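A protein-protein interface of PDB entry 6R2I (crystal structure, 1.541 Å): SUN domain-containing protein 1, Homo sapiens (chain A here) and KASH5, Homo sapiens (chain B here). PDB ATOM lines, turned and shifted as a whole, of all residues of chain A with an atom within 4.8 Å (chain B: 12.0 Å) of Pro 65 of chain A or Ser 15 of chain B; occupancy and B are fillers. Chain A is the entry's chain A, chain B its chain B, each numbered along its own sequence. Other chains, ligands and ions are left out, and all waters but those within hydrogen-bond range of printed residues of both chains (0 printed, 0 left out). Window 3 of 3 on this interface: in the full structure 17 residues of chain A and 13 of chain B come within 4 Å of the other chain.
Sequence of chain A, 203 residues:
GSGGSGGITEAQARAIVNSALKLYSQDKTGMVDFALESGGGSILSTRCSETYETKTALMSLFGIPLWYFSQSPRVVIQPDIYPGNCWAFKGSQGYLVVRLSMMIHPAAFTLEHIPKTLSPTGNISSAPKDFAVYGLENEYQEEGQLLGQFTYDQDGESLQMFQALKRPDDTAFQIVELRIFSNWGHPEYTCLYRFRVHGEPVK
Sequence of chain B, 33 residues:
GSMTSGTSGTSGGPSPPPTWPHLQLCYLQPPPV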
ATOM      1  N   LEU A  58      -8.270  -1.088 -21.835  1.00  0.00           N
ATOM      2  CA  LEU A  58      -7.225  -0.926 -22.840  1.00  0.00           C
ATOM      3  C   LEU A  58      -6.491   0.386 -22.592  1.00  0.00           C
ATOM      4  O   LEU A  58      -7.121   1.450 -22.513  1.00  0.00           O
ATOM      5  CB  LEU A  58      -7.821  -0.949 -24.248  1.00  0.00           C
ATOM      6  CG  LEU A  58      -6.865  -0.704 -25.418  1.00  0.00           C
ATOM      7  CD1 LEU A  58      -5.811  -1.782 -25.481  1.00  0.00           C
ATOM      8  CD2 LEU A  58      -7.625  -0.640 -26.734  1.00  0.00           C
ATOM      9  N   MET A  59      -5.168   0.303 -22.451  1.00  0.00           N
ATOM     10  CA  MET A  59      -4.305   1.457 -22.273  1.00  0.00           C
ATOM     11  C   MET A  59      -3.620   1.780 -23.589  1.00  0.00           C
ATOM     12  O   MET A  59      -3.071   0.876 -24.248  1.00  0.00           O
ATOM     13  CB  MET A  59      -3.229   1.212 -21.216  1.00  0.00           C
ATOM     14  CG  MET A  59      -3.728   0.762 -19.868  1.00  0.00           C
ATOM     15  SD  MET A  59      -4.824   1.948 -19.076  1.00  0.00           S
ATOM     16  CE  MET A  59      -3.756   3.375 -18.914  1.00  0.00           C
ATOM     17  N   SER A  60      -3.611   3.071 -23.924  1.00  0.00           N
ATOM     18  CA  SER A  60      -3.078   3.589 -25.170  1.00  0.00           C
ATOM     19  C   SER A  60      -2.121   4.739 -24.894  1.00  0.00           C
ATOM     20  O   SER A  60      -2.157   5.380 -23.840  1.00  0.00           O
ATOM     21  CB  SER A  60      -4.191   4.085 -26.103  1.00  0.00           C
ATOM     22  OG  SER A  60      -5.123   3.057 -26.378  1.00  0.00           O
ATOM     23  N   GLY A  63      -2.408   7.169 -29.282  1.00  0.00           N
ATOM     24  CA  GLY A  63      -3.551   6.767 -30.075  1.00  0.00           C
ATOM     25  C   GLY A  63      -3.630   5.301 -30.448  1.00  0.00           C
ATOM     26  O   GLY A  63      -4.680   4.868 -30.942  1.00  0.00           O
ATOM     27  N   ILE A  64      -2.575   4.523 -30.231  1.00  0.00           N
ATOM     28  CA  ILE A  64      -2.545   3.143 -30.719  1.00  0.00           C
ATOM     29  C   ILE A  64      -2.657   2.175 -29.548  1.00  0.00           C
ATOM     30  O   ILE A  64      -2.032   2.392 -28.501  1.00  0.00           O
ATOM     31  CB  ILE A  64      -1.276   2.891 -31.552  1.00  0.00           C
ATOM     32  CG1 ILE A  64      -1.367   3.706 -32.845  1.00  0.00           C
ATOM     33  CG2 ILE A  64      -1.102   1.403 -31.861  1.00  0.00           C
ATOM     34  CD1 ILE A  64      -0.137   3.670 -33.702  1.00  0.00           C
ATOM     35  N   PRO A  65      -3.439   1.101 -29.677  1.00  0.00           N
ATOM     36  CA  PRO A  65      -3.548   0.127 -28.583  1.00  0.00           C
ATOM     37  C   PRO A  65      -2.177  -0.336 -28.110  1.00  0.00           C
ATOM     38  O   PRO A  65      -1.319  -0.717 -28.912  1.00  0.00           O
ATOM     39  CB  PRO A  65      -4.349  -1.020 -29.208  1.00  0.00           C
ATOM     40  CG  PRO A  65      -5.097  -0.407 -30.340  1.00  0.00           C
ATOM     41  CD  PRO A  65      -4.285   0.745 -30.833  1.00  0.00           C
ATOM     42  N   LEU A  66      -1.972  -0.303 -26.792  1.00  0.00           N
ATOM     43  CA  LEU A  66      -0.691  -0.658 -26.196  1.00  0.00           C
ATOM     44  C   LEU A  66      -0.758  -1.876 -25.296  1.00  0.00           C
ATOM     45  O   LEU A  66       0.071  -2.785 -25.437  1.00  0.00           O
ATOM     46  CB  LEU A  66      -0.133   0.487 -25.370  1.00  0.00           C
ATOM     47  CG  LEU A  66       0.166   1.806 -26.042  1.00  0.00           C
ATOM     48  CD1 LEU A  66       0.697   2.643 -24.919  1.00  0.00           C
ATOM     49  CD2 LEU A  66       1.158   1.669 -27.180  1.00  0.00           C
ATOM     50  N   TRP A  67      -1.689  -1.912 -24.344  1.00  0.00           N
ATOM     51  CA  TRP A  67      -1.809  -3.142 -23.563  1.00  0.00           C
ATOM     52  C   TRP A  67      -3.080  -3.115 -22.737  1.00  0.00           C
ATOM     53  O   TRP A  67      -3.630  -2.053 -22.461  1.00  0.00           O
ATOM     54  CB  TRP A  67      -0.594  -3.371 -22.657  1.00  0.00           C
ATOM     55  CG  TRP A  67      -0.012  -2.146 -22.019  1.00  0.00           C
ATOM     56  CD1 TRP A  67       0.961  -1.338 -22.534  1.00  0.00           C
ATOM     57  CD2 TRP A  67      -0.338  -1.610 -20.732  1.00  0.00           C
ATOM     58  NE1 TRP A  67       1.252  -0.327 -21.648  1.00  0.00           N
ATOM     59  CE2 TRP A  67       0.467  -0.473 -20.535  1.00  0.00           C
ATOM     60  CE3 TRP A  67      -1.242  -1.974 -19.734  1.00  0.00           C
ATOM     61  CZ2 TRP A  67       0.398   0.297 -19.376  1.00  0.00           C
ATOM     62  CZ3 TRP A  67      -1.301  -1.220 -18.581  1.00  0.00           C
ATOM     63  CH2 TRP A  67      -0.492  -0.091 -18.414  1.00  0.00           C
ATOM     64  N   SER B  15      -6.976  -2.135 -32.813  1.00  0.00           N
ATOM     65  CA  SER B  15      -6.214  -3.380 -32.807  1.00  0.00           C
ATOM     66  C   SER B  15      -5.992  -3.859 -31.368  1.00  0.00           C
ATOM     67  O   SER B  15      -6.223  -3.108 -30.422  1.00  0.00           O
ATOM     68  CB  SER B  15      -4.879  -3.189 -33.531  1.00  0.00           C
ATOM     69  OG  SER B  15      -4.153  -2.100 -32.990  1.00  0.00           O
ATOM     70  N   PRO B  16      -5.575  -5.113 -31.200  1.00  0.00           N
ATOM     71  CA  PRO B  16      -5.367  -5.652 -29.853  1.00  0.00           C
ATOM     72  C   PRO B  16      -3.912  -5.548 -29.430  1.00  0.00           C
ATOM     73  O   PRO B  16      -3.010  -5.849 -30.223  1.00  0.00           O
ATOM     74  CB  PRO B  16      -5.794  -7.121 -30.007  1.00  0.00           C
ATOM     75  CG  PRO B  16      -5.534  -7.441 -31.489  1.00  0.00           C
ATOM     76  CD  PRO B  16      -5.303  -6.134 -32.227  1.00  0.00           C
ATOM     77  N   PRO B  17      -3.634  -5.108 -28.202  1.00  0.00           N
ATOM     78  CA  PRO B  17      -2.283  -5.266 -27.618  1.00  0.00           C
ATOM     79  C   PRO B  17      -2.187  -6.480 -26.706  1.00  0.00           C
ATOM     80  O   PRO B  17      -3.129  -7.285 -26.642  1.00  0.00           O
ATOM     81  CB  PRO B  17      -2.096  -3.961 -26.846  1.00  0.00           C
ATOM     82  CG  PRO B  17      -3.486  -3.495 -26.517  1.00  0.00           C
ATOM     83  CD  PRO B  17      -4.487  -4.283 -27.335  1.00  0.00           C
ATOM     84  N   PRO B  18      -1.058  -6.676 -26.001  1.00  0.00           N
ATOM     85  CA  PRO B  18      -0.978  -7.740 -24.992  1.00  0.00           C
ATOM     86  C   PRO B  18      -1.548  -7.303 -23.644  1.00  0.00           C
ATOM     87  O   PRO B  18      -2.084  -6.208 -23.486  1.00  0.00           O
ATOM     88  CB  PRO B  18       0.528  -7.996 -24.889  1.00  0.00           C
ATOM     89  CG  PRO B  18       1.107  -6.661 -25.083  1.00  0.00           C
ATOM     90  CD  PRO B  18       0.266  -6.048 -26.182  1.00  0.00           C
ATOM     91  N   THR B  19      -1.412  -8.192 -22.659  1.00  0.00           N
ATOM     92  CA  THR B  19      -1.840  -7.934 -21.289  1.00  0.00           C
ATOM     93  C   THR B  19      -0.641  -7.515 -20.449  1.00  0.00           C
ATOM     94  O   THR B  19       0.403  -8.176 -20.477  1.00  0.00           O
ATOM     95  CB  THR B  19      -2.492  -9.171 -20.663  1.00  0.00           C
ATOM     96  OG1 THR B  19      -3.762  -9.418 -21.279  1.00  0.00           O
ATOM     97  CG2 THR B  19      -2.680  -8.982 -19.155  1.00  0.00           C
ATOM     98  N   TRP B  20      -0.796  -6.436 -19.700  1.00  0.00           N
ATOM     99  CA  TRP B  20       0.276  -5.980 -18.830  1.00  0.00           C
ATOM    100  C   TRP B  20       0.466  -6.986 -17.710  1.00  0.00           C
ATOM    101  O   TRP B  20      -0.393  -7.073 -16.823  1.00  0.00           O
ATOM    102  CB  TRP B  20      -0.041  -4.609 -18.244  1.00  0.00           C
ATOM    103  CG  TRP B  20       1.165  -3.877 -17.700  1.00  0.00           C
ATOM    104  CD1 TRP B  20       2.363  -3.690 -18.328  1.00  0.00           C
ATOM    105  CD2 TRP B  20       1.275  -3.221 -16.427  1.00  0.00           C
ATOM    106  NE1 TRP B  20       3.213  -2.969 -17.525  1.00  0.00           N
ATOM    107  CE2 TRP B  20       2.570  -2.666 -16.354  1.00  0.00           C
ATOM    108  CE3 TRP B  20       0.407  -3.049 -15.343  1.00  0.00           C
ATOM    109  CZ2 TRP B  20       3.017  -1.956 -15.241  1.00  0.00           C
ATOM    110  CZ3 TRP B  20       0.855  -2.343 -14.238  1.00  0.00           C
ATOM    111  CH2 TRP B  20       2.147  -1.806 -14.197  1.00  0.00           C
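O of Met 59 of chain A is in hydrogen-bond range of N of Leu 66 of chain A (3.0 Å).
N of Met 59 of chain A lies within hydrogen-bond range of O of Trp 67 of chain A.
Of the printed residues of chain B, Pro 65 of chain A touches Ser 15 and Pro 17.
Ser 15 of chain B touches one residue of chain A.
No residue of chain B comes within 4 Å of Ser 60 of chain A.
No residue of chain B comes within 4 Å of Gly 63 of chain A.
Of the printed residues of chain A, Trp 20 of chain B touches Trp 67.
Of the printed residues of chain A, Pro 18 of chain B touches Leu 66 (3.4 Å) and Trp 67 (3.1 Å).
Of the printed residues of chain B, Trp 67 of chain A touches Pro 17, Pro 18 and Trp 20.
Pro 16 of chain B touches none of the printed residues of chain A.
Thr 19 of chain B touches none of the printed residues of chain A.
The nearest residue of chain A that does not touch Ser 15 of chain B is Leu 58 of chain A (4.7 Å).
Of the 8 printed residues of chain A, 4 touch a printed residue of chain B.
Of the 6 printed residues of chain B, 4 touch a printed residue of chain A.
Hydrophobic or aromatic side chains of chain B that line the printed part of chain A: Pro 17, Pro 18 and Trp 20.
Among the printed residues, no Asp or Glu carboxylate lies within 4 Å of a Lys or Arg side-chain nitrogen of the other chain.
Among the printed residues, pairs that only touch across the chains: Leu 58 of chain A with Pro 17 of chain B (3.1 Å), Pro 65 of chain A with Ser 15 of chain B (2.9 Å), Pro 65 of chain A with Pro 17 of chain B (3.8 Å), Leu 66 of chain A with Pro 17 of chain B (2.8 Å), Leu 66 of chain A with Pro 18 of chain B (3.4 Å), Trp 67 of chain A with Pro 17 of chain B (3.2 Å), Trp 67 of chain A with Pro 18 of chain B (3.1 Å) and Trp 67 of chain A with Trp 20 of chain B (3.3 Å).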
